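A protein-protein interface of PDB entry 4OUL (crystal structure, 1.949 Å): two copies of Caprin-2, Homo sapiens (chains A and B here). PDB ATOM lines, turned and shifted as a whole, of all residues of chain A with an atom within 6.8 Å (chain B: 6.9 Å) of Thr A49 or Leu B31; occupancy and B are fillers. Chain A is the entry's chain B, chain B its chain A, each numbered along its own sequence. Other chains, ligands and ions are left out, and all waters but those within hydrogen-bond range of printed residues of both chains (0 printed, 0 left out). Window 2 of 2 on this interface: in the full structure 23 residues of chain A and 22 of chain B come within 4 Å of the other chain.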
ATOM      1  N   VAL A  46      16.963 -25.593 -24.627  1.00  0.00           N
ATOM      2  CA  VAL A  46      18.086 -25.484 -23.713  1.00  0.00           C
ATOM      3  C   VAL A  46      17.751 -24.568 -22.542  1.00  0.00           C
ATOM      4  O   VAL A  46      16.976 -23.617 -22.671  1.00  0.00           O
ATOM      5  CB  VAL A  46      19.360 -24.966 -24.451  1.00  0.00           C
ATOM      6  CG1 VAL A  46      19.154 -23.548 -24.978  1.00  0.00           C
ATOM      7  CG2 VAL A  46      20.596 -25.050 -23.554  1.00  0.00           C
ATOM      8  N   ASN A  47      18.302 -24.893 -21.381  1.00  0.00           N
ATOM      9  CA  ASN A  47      18.190 -24.028 -20.218  1.00  0.00           C
ATOM     10  C   ASN A  47      18.731 -22.636 -20.526  1.00  0.00           C
ATOM     11  O   ASN A  47      19.831 -22.496 -21.067  1.00  0.00           O
ATOM     12  CB  ASN A  47      18.935 -24.650 -19.043  1.00  0.00           C
ATOM     13  CG  ASN A  47      18.360 -25.996 -18.644  1.00  0.00           C
ATOM     14  OD1 ASN A  47      17.464 -26.533 -19.311  1.00  0.00           O
ATOM     15  ND2 ASN A  47      18.899 -26.570 -17.574  1.00  0.00           N
ATOM     16  N   GLY A  48      17.967 -21.606 -20.168  1.00  0.00           N
ATOM     17  CA  GLY A  48      18.413 -20.243 -20.385  1.00  0.00           C
ATOM     18  C   GLY A  48      17.318 -19.222 -20.127  1.00  0.00           C
ATOM     19  O   GLY A  48      16.238 -19.585 -19.684  1.00  0.00           O
ATOM     20  N   THR A  49      17.623 -17.953 -20.384  1.00  0.00           N
ATOM     21  CA  THR A  49      16.679 -16.846 -20.194  1.00  0.00           C
ATOM     22  C   THR A  49      16.011 -16.478 -21.504  1.00  0.00           C
ATOM     23  O   THR A  49      16.702 -16.196 -22.482  1.00  0.00           O
ATOM     24  CB  THR A  49      17.381 -15.600 -19.634  1.00  0.00           C
ATOM     25  OG1 THR A  49      18.200 -15.966 -18.516  1.00  0.00           O
ATOM     26  CG2 THR A  49      16.351 -14.542 -19.215  1.00  0.00           C
ATOM     27  N   TYR A  50      14.675 -16.429 -21.504  1.00  0.00           N
ATOM     28  CA  TYR A  50      13.888 -16.218 -22.712  1.00  0.00           C
ATOM     29  C   TYR A  50      12.920 -15.037 -22.597  1.00  0.00           C
ATOM     30  O   TYR A  50      12.426 -14.744 -21.506  1.00  0.00           O
ATOM     31  CB  TYR A  50      13.083 -17.482 -23.042  1.00  0.00           C
ATOM     32  CG  TYR A  50      13.927 -18.674 -23.448  1.00  0.00           C
ATOM     33  CD1 TYR A  50      14.599 -19.431 -22.493  1.00  0.00           C
ATOM     34  CD2 TYR A  50      14.047 -19.042 -24.781  1.00  0.00           C
ATOM     35  CE1 TYR A  50      15.368 -20.523 -22.857  1.00  0.00           C
ATOM     36  CE2 TYR A  50      14.820 -20.130 -25.156  1.00  0.00           C
ATOM     37  CZ  TYR A  50      15.465 -20.870 -24.190  1.00  0.00           C
ATOM     38  OH  TYR A  50      16.225 -21.957 -24.559  1.00  0.00           O
ATOM     39  N   VAL A  51      12.663 -14.397 -23.736  1.00  0.00           N
ATOM     40  CA  VAL A  51      11.717 -13.288 -23.866  1.00  0.00           C
ATOM     41  C   VAL A  51      10.518 -13.727 -24.723  1.00  0.00           C
ATOM     42  O   VAL A  51      10.706 -14.384 -25.747  1.00  0.00           O
ATOM     43  CB  VAL A  51      12.400 -12.049 -24.517  1.00  0.00           C
ATOM     44  CG1 VAL A  51      11.398 -10.873 -24.668  1.00  0.00           C
ATOM     45  CG2 VAL A  51      13.641 -11.624 -23.729  1.00  0.00           C
ATOM     46  N   ILE A  96       9.901 -12.050 -19.416  1.00  0.00           N
ATOM     47  CA  ILE A  96      11.275 -12.540 -19.476  1.00  0.00           C
ATOM     48  C   ILE A  96      11.469 -13.503 -18.315  1.00  0.00           C
ATOM     49  O   ILE A  96      11.246 -13.160 -17.153  1.00  0.00           O
ATOM     50  CB  ILE A  96      12.292 -11.409 -19.406  1.00  0.00           C
ATOM     51  CG1 ILE A  96      11.965 -10.345 -20.471  1.00  0.00           C
ATOM     52  CG2 ILE A  96      13.718 -11.952 -19.594  1.00  0.00           C
ATOM     53  CD1 ILE A  96      12.939  -9.200 -20.505  1.00  0.00           C
ATOM     54  N   LEU A  97      11.834 -14.736 -18.633  1.00  0.00           N
ATOM     55  CA  LEU A  97      11.891 -15.787 -17.626  1.00  0.00           C
ATOM     56  C   LEU A  97      12.983 -16.807 -17.892  1.00  0.00           C
ATOM     57  O   LEU A  97      13.330 -17.058 -19.042  1.00  0.00           O
ATOM     58  CB  LEU A  97      10.508 -16.429 -17.506  1.00  0.00           C
ATOM     59  CG  LEU A  97       9.815 -16.490 -18.867  1.00  0.00           C
ATOM     60  CD1 LEU A  97      10.108 -17.730 -19.631  1.00  0.00           C
ATOM     61  CD2 LEU A  97       8.332 -16.313 -18.672  1.00  0.00           C
ATOM     62  N   GLN A  98      13.512 -17.376 -16.816  1.00  0.00           N
ATOM     63  CA  GLN A  98      14.410 -18.527 -16.907  1.00  0.00           C
ATOM     64  C   GLN A  98      13.622 -19.804 -17.189  1.00  0.00           C
ATOM     65  O   GLN A  98      12.636 -20.097 -16.507  1.00  0.00           O
ATOM     66  CB  GLN A  98      15.223 -18.674 -15.621  1.00  0.00           C
ATOM     67  N   LEU A  99      14.029 -20.529 -18.229  1.00  0.00           N
ATOM     68  CA  LEU A  99      13.394 -21.793 -18.580  1.00  0.00           C
ATOM     69  C   LEU A  99      14.354 -22.972 -18.526  1.00  0.00           C
ATOM     70  O   LEU A  99      15.566 -22.820 -18.721  1.00  0.00           O
ATOM     71  CB  LEU A  99      12.793 -21.714 -19.984  1.00  0.00           C
ATOM     72  CG  LEU A  99      11.612 -20.752 -20.125  1.00  0.00           C
ATOM     73  CD1 LEU A  99      11.040 -20.803 -21.546  1.00  0.00           C
ATOM     74  CD2 LEU A  99      10.555 -21.118 -19.096  1.00  0.00           C
ATOM     75  N   TYR A 127      12.265 -15.564 -27.993  1.00  0.00           N
ATOM     76  CA  TYR A 127      13.648 -15.857 -28.345  1.00  0.00           C
ATOM     77  C   TYR A 127      14.523 -16.056 -27.134  1.00  0.00           C
ATOM     78  O   TYR A 127      14.175 -15.659 -26.029  1.00  0.00           O
ATOM     79  CB  TYR A 127      14.233 -14.750 -29.220  1.00  0.00           C
ATOM     80  CG  TYR A 127      14.252 -13.375 -28.592  1.00  0.00           C
ATOM     81  CD1 TYR A 127      13.143 -12.542 -28.673  1.00  0.00           C
ATOM     82  CD2 TYR A 127      15.377 -12.907 -27.936  1.00  0.00           C
ATOM     83  CE1 TYR A 127      13.157 -11.288 -28.121  1.00  0.00           C
ATOM     84  CE2 TYR A 127      15.399 -11.652 -27.377  1.00  0.00           C
ATOM     85  CZ  TYR A 127      14.288 -10.847 -27.481  1.00  0.00           C
ATOM     86  OH  TYR A 127      14.296  -9.595 -26.924  1.00  0.00           O
ATOM     87  N   LEU A 128      15.672 -16.692 -27.359  1.00  0.00           N
ATOM     88  CA  LEU A 128      16.637 -16.933 -26.311  1.00  0.00           C
ATOM     89  C   LEU A 128      17.529 -15.709 -26.148  1.00  0.00           C
ATOM     90  O   LEU A 128      18.203 -15.303 -27.097  1.00  0.00           O
ATOM     91  CB  LEU A 128      17.485 -18.184 -26.646  1.00  0.00           C
ATOM     92  CG  LEU A 128      18.648 -18.450 -25.705  1.00  0.00           C
ATOM     93  CD1 LEU A 128      18.150 -18.742 -24.294  1.00  0.00           C
ATOM     94  CD2 LEU A 128      19.532 -19.601 -26.229  1.00  0.00           C
ATOM     95  N   LEU A 129      17.538 -15.129 -24.953  1.00  0.00           N
ATOM     96  CA  LEU A 129      18.401 -13.991 -24.659  1.00  0.00           C
ATOM     97  C   LEU A 129      19.771 -14.476 -24.186  1.00  0.00           C
ATOM     98  O   LEU A 129      20.800 -14.154 -24.781  1.00  0.00           O
ATOM     99  CB  LEU A 129      17.772 -13.078 -23.596  1.00  0.00           C
ATOM    100  N   TYR A 130      19.772 -15.271 -23.121  1.00  0.00           N
ATOM    101  CA  TYR A 130      21.012 -15.752 -22.526  1.00  0.00           C
ATOM    102  C   TYR A 130      20.929 -17.246 -22.301  1.00  0.00           C
ATOM    103  O   TYR A 130      20.000 -17.717 -21.651  1.00  0.00           O
ATOM    104  CB  TYR A 130      21.274 -15.081 -21.187  1.00  0.00           C
ATOM    105  CG  TYR A 130      21.304 -13.571 -21.208  1.00  0.00           C
ATOM    106  CD1 TYR A 130      22.182 -12.883 -22.024  1.00  0.00           C
ATOM    107  CD2 TYR A 130      20.455 -12.840 -20.391  1.00  0.00           C
ATOM    108  CE1 TYR A 130      22.211 -11.503 -22.025  1.00  0.00           C
ATOM    109  CE2 TYR A 130      20.477 -11.472 -20.379  1.00  0.00           C
ATOM    110  CZ  TYR A 130      21.358 -10.805 -21.199  1.00  0.00           C
ATOM    111  OH  TYR A 130      21.387  -9.430 -21.196  1.00  0.00           O
ATOM    112  N   GLN A 131      21.886 -18.000 -22.825  1.00  0.00           N
ATOM    113  CA  GLN A 131      21.912 -19.434 -22.553  1.00  0.00           C
ATOM    114  C   GLN A 131      22.468 -19.655 -21.127  1.00  0.00           C
ATOM    115  O   GLN A 131      23.335 -18.909 -20.691  1.00  0.00           O
ATOM    116  CB  GLN A 131      22.727 -20.145 -23.631  1.00  0.00           C
ATOM    117  CG  GLN A 131      22.582 -21.657 -23.639  1.00  0.00           C
ATOM    118  CD  GLN A 131      23.576 -22.305 -24.570  1.00  0.00           C
ATOM    119  OE1 GLN A 131      23.202 -22.888 -25.590  1.00  0.00           O
ATOM    120  NE2 GLN A 131      24.860 -22.193 -24.236  1.00  0.00           N
ATOM    121  N   ASP A 132      21.940 -20.673 -20.441  1.00  0.00           N
ATOM    122  CA  ASP A 132      22.198 -21.080 -19.035  1.00  0.00           C
ATOM    123  C   ASP A 132      21.050 -20.594 -18.147  1.00  0.00           C
ATOM    124  O   ASP A 132      20.752 -21.201 -17.115  1.00  0.00           O
ATOM    125  CB  ASP A 132      23.528 -20.582 -18.440  1.00  0.00           C
ATOM    126  CG  ASP A 132      24.744 -21.255 -19.051  1.00  0.00           C
ATOM    127  OD1 ASP A 132      24.583 -22.334 -19.659  1.00  0.00           O
ATOM    128  OD2 ASP A 132      25.865 -20.731 -18.865  1.00  0.00           O
ATOM    129  N   ARG B   2      25.423  -9.831 -18.244  1.00  0.00           N
ATOM    130  CA  ARG B   2      24.078 -10.407 -18.375  1.00  0.00           C
ATOM    131  C   ARG B   2      23.081  -9.876 -17.352  1.00  0.00           C
ATOM    132  O   ARG B   2      23.208 -10.140 -16.153  1.00  0.00           O
ATOM    133  CB  ARG B   2      24.132 -11.928 -18.260  1.00  0.00           C
ATOM    134  CG  ARG B   2      24.474 -12.599 -19.560  1.00  0.00           C
ATOM    135  CD  ARG B   2      24.446 -14.106 -19.448  1.00  0.00           C
ATOM    136  NE  ARG B   2      24.922 -14.714 -20.682  1.00  0.00           N
ATOM    137  CZ  ARG B   2      25.034 -16.020 -20.875  1.00  0.00           C
ATOM    138  NH1 ARG B   2      24.695 -16.862 -19.908  1.00  0.00           N
ATOM    139  NH2 ARG B   2      25.471 -16.476 -22.039  1.00  0.00           N
ATOM    140  N   VAL B   3      22.122  -9.076 -17.823  1.00  0.00           N
ATOM    141  CA  VAL B   3      21.144  -8.440 -16.939  1.00  0.00           C
ATOM    142  C   VAL B   3      19.725  -8.510 -17.556  1.00  0.00           C
ATOM    143  O   VAL B   3      19.529  -8.256 -18.748  1.00  0.00           O
ATOM    144  CB  VAL B   3      21.544  -6.972 -16.556  1.00  0.00           C
ATOM    145  CG1 VAL B   3      23.054  -6.857 -16.305  1.00  0.00           C
ATOM    146  CG2 VAL B   3      21.103  -5.970 -17.583  1.00  0.00           C
ATOM    147  N   ALA B   4      18.763  -8.962 -16.762  1.00  0.00           N
ATOM    148  CA  ALA B   4      17.362  -9.043 -17.198  1.00  0.00           C
ATOM    149  C   ALA B   4      16.450  -9.109 -15.995  1.00  0.00           C
ATOM    150  O   ALA B   4      16.706  -9.836 -15.041  1.00  0.00           O
ATOM    151  CB  ALA B   4      17.132 -10.248 -18.095  1.00  0.00           C
ATOM    152  N   PHE B   5      15.400  -8.305 -16.015  1.00  0.00           N
ATOM    153  CA  PHE B   5      14.416  -8.376 -14.962  1.00  0.00           C
ATOM    154  C   PHE B   5      13.018  -8.419 -15.577  1.00  0.00           C
ATOM    155  O   PHE B   5      12.812  -8.034 -16.724  1.00  0.00           O
ATOM    156  CB  PHE B   5      14.574  -7.200 -13.988  1.00  0.00           C
ATOM    157  CG  PHE B   5      14.212  -5.879 -14.573  1.00  0.00           C
ATOM    158  CD1 PHE B   5      15.163  -5.115 -15.230  1.00  0.00           C
ATOM    159  CD2 PHE B   5      12.915  -5.397 -14.478  1.00  0.00           C
ATOM    160  CE1 PHE B   5      14.826  -3.899 -15.783  1.00  0.00           C
ATOM    161  CE2 PHE B   5      12.579  -4.192 -15.024  1.00  0.00           C
ATOM    162  CZ  PHE B   5      13.522  -3.442 -15.677  1.00  0.00           C
ATOM    163  N   SER B   6      12.070  -8.910 -14.804  1.00  0.00           N
ATOM    164  CA  SER B   6      10.685  -8.930 -15.232  1.00  0.00           C
ATOM    165  C   SER B   6       9.884  -8.828 -13.955  1.00  0.00           C
ATOM    166  O   SER B   6      10.044  -9.657 -13.064  1.00  0.00           O
ATOM    167  CB  SER B   6      10.377 -10.209 -16.021  1.00  0.00           C
ATOM    168  OG  SER B   6       9.156 -10.109 -16.718  1.00  0.00           O
ATOM    169  N   ASN B  29      11.895 -12.530 -12.842  1.00  0.00           N
ATOM    170  CA  ASN B  29      13.304 -12.773 -13.188  1.00  0.00           C
ATOM    171  C   ASN B  29      14.157 -11.634 -12.688  1.00  0.00           C
ATOM    172  O   ASN B  29      13.685 -10.508 -12.650  1.00  0.00           O
ATOM    173  CB  ASN B  29      13.467 -12.894 -14.686  1.00  0.00           C
ATOM    174  CG  ASN B  29      14.782 -13.519 -15.093  1.00  0.00           C
ATOM    175  OD1 ASN B  29      15.698 -13.658 -14.293  1.00  0.00           O
ATOM    176  ND2 ASN B  29      14.872 -13.913 -16.358  1.00  0.00           N
ATOM    177  N   ASN B  30      15.398 -11.875 -12.309  1.00  0.00           N
ATOM    178  CA  ASN B  30      16.175 -10.717 -11.959  1.00  0.00           C
ATOM    179  C   ASN B  30      17.634 -11.020 -12.235  1.00  0.00           C
ATOM    180  O   ASN B  30      18.486 -10.918 -11.333  1.00  0.00           O
ATOM    181  CB  ASN B  30      16.092 -10.395 -10.480  1.00  0.00           C
ATOM    182  CG  ASN B  30      16.162  -8.885 -10.228  1.00  0.00           C
ATOM    183  OD1 ASN B  30      15.682  -8.140 -11.103  1.00  0.00           O
ATOM    184  ND2 ASN B  30      16.844  -8.429  -9.169  1.00  0.00           N
ATOM    185  N   LEU B  31      17.909 -11.489 -13.441  1.00  0.00           N
ATOM    186  CA  LEU B  31      19.262 -11.835 -13.827  1.00  0.00           C
ATOM    187  C   LEU B  31      20.202 -10.632 -13.698  1.00  0.00           C
ATOM    188  O   LEU B  31      20.063  -9.630 -14.397  1.00  0.00           O
ATOM    189  CB  LEU B  31      19.262 -12.379 -15.238  1.00  0.00           C
ATOM    190  CG  LEU B  31      20.611 -12.869 -15.696  1.00  0.00           C
ATOM    191  CD1 LEU B  31      21.071 -13.993 -14.771  1.00  0.00           C
ATOM    192  CD2 LEU B  31      20.457 -13.398 -17.091  1.00  0.00           C
ATOM    193  N   GLY B  32      21.130 -10.742 -12.746  1.00  0.00           N
ATOM    194  CA  GLY B  32      22.124  -9.715 -12.484  1.00  0.00           C
ATOM    195  C   GLY B  32      21.839  -8.941 -11.209  1.00  0.00           C
ATOM    196  O   GLY B  32      22.592  -8.038 -10.842  1.00  0.00           O
ATOM    197  N   GLU B  33      20.707  -9.268 -10.585  1.00  0.00           N
ATOM    198  CA  GLU B  33      20.174  -8.659  -9.365  1.00  0.00           C
ATOM    199  C   GLU B  33      20.184  -7.141  -9.362  1.00  0.00           C
ATOM    200  O   GLU B  33      20.547  -6.476  -8.385  1.00  0.00           O
ATOM    201  CB  GLU B  33      20.892  -9.234  -8.148  1.00  0.00           C
ATOM    202  CG  GLU B  33      21.165 -10.739  -8.332  1.00  0.00           C
ATOM    203  CD  GLU B  33      21.775 -11.376  -7.111  1.00  0.00           C
ATOM    204  OE1 GLU B  33      21.092 -12.237  -6.504  1.00  0.00           O
ATOM    205  OE2 GLU B  33      22.889 -10.960  -6.726  1.00  0.00           O
ATOM    206  N   THR B  34      19.717  -6.612 -10.486  1.00  0.00           N
ATOM    207  CA  THR B  34      19.542  -5.188 -10.658  1.00  0.00           C
ATOM    208  C   THR B  34      18.085  -5.066 -10.307  1.00  0.00           C
ATOM    209  O   THR B  34      17.458  -6.084 -10.041  1.00  0.00           O
ATOM    210  CB  THR B  34      19.798  -4.694 -12.098  1.00  0.00           C
ATOM    211  OG1 THR B  34      18.768  -5.169 -12.981  1.00  0.00           O
ATOM    212  CG2 THR B  34      21.158  -5.150 -12.614  1.00  0.00           C
ATOM    213  N   PHE B  42      15.219   0.145 -11.673  1.00  0.00           N
ATOM    214  CA  PHE B  42      16.326  -0.613 -12.246  1.00  0.00           C
ATOM    215  C   PHE B  42      17.601   0.204 -12.066  1.00  0.00           C
ATOM    216  O   PHE B  42      17.643   1.388 -12.390  1.00  0.00           O
ATOM    217  CB  PHE B  42      16.057  -0.932 -13.715  1.00  0.00           C
ATOM    218  CG  PHE B  42      17.272  -1.320 -14.508  1.00  0.00           C
ATOM    219  CD1 PHE B  42      17.833  -2.580 -14.382  1.00  0.00           C
ATOM    220  CD2 PHE B  42      17.815  -0.439 -15.436  1.00  0.00           C
ATOM    221  CE1 PHE B  42      18.935  -2.947 -15.139  1.00  0.00           C
ATOM    222  CE2 PHE B  42      18.916  -0.797 -16.199  1.00  0.00           C
ATOM    223  CZ  PHE B  42      19.476  -2.053 -16.052  1.00  0.00           C
ATOM    224  N   GLY B 126      13.180  -5.514 -18.455  1.00  0.00           N
ATOM    225  CA  GLY B 126      14.266  -4.867 -19.149  1.00  0.00           C
ATOM    226  C   GLY B 126      15.438  -5.826 -19.247  1.00  0.00           C
ATOM    227  O   GLY B 126      15.556  -6.745 -18.446  1.00  0.00           O
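No position is printed for both chains. Of the 11 pairs that touch across the chains among the printed residues, none has its exchanged pair printed and touching as well.
Hydrophobic or aromatic side chains of chain A within 4 Å of the printed part of chain B: Ile A96 and Tyr A130. Among the printed residues, 11 pairs touch across the chains. Among the printed residues, no Asp or Glu carboxylate lies within 4 Å of a Lys or Arg side-chain nitrogen of the other chain.
NH1 of Arg B2 lies within hydrogen-bond range of O of Gln A131 (2.6 Å). O of Val B3 sits at hydrogen-bond distance from OH of Tyr A130. N of Ile A96 is in hydrogen-bond range of OG of Ser B6 (3.4 Å).
The backbone carbonyl oxygen of Thr A49 lies within hydrogen-bond range of the backbone NH of Leu A129 (2.8 Å). The backbone NH (N) of Thr A49 lies within hydrogen-bond range of the backbone carbonyl oxygen (O) of Tyr A130. The backbone NH of Ser B6 is in hydrogen-bond range of the backbone carbonyl oxygen of Asn B29, at 3.1 Å. O of Leu A97 sits at hydrogen-bond distance from N of Tyr A50 (2.9 Å). N of Leu B31 is in hydrogen-bond range of OD1 of Asn B29, 3.2 Å away. N of Leu B31 lies within hydrogen-bond range of O of Ala B4, at 2.6 Å.
Of the printed residues of chain B, Thr A49 touches Asn B29 (3.3 Å) and Leu B31 (3.7 Å). Of chain A, only Thr A49 and Tyr A130 come within 4 Å of Leu B31. Printed residues of chain B within 4 Å of Leu A97: Asn B29. Of the printed residues of chain B, Gln A98 touches Asn B29 (3.7 Å). Of the printed residues of chain A, Arg B2 touches Tyr A130 (3.4 Å) and Gln A131 (2.6 Å). Printed residues of chain B within 4 Å of Gln A131: Arg B2. Asn B30 touches none of the printed residues of chain A. The nearest residue of chain B that does not touch Thr A49 is Ala B4 (4.5 Å). The nearest printed residue of chain A that does not touch Leu B31 is Leu A129 (7.0 Å). The nearest printed residue of chain A that does not touch Arg B2 is Asp A132 (4.2 Å).
Among the printed residues, merely in contact across the chains: Thr A49 with Asn B29 (3.3 Å), Thr A49 with Leu B31 (3.7 Å), Ile A96 with Phe B5 (3.96 Å), Ile A96 with Asn B29 (3.3 Å), Leu A97 with Asn B29 (3.7 Å), Gln A98 with Asn B29 (3.7 Å), Tyr A130 with Arg B2 (3.4 Å) and Tyr A130 with Leu B31 (3.3 Å).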
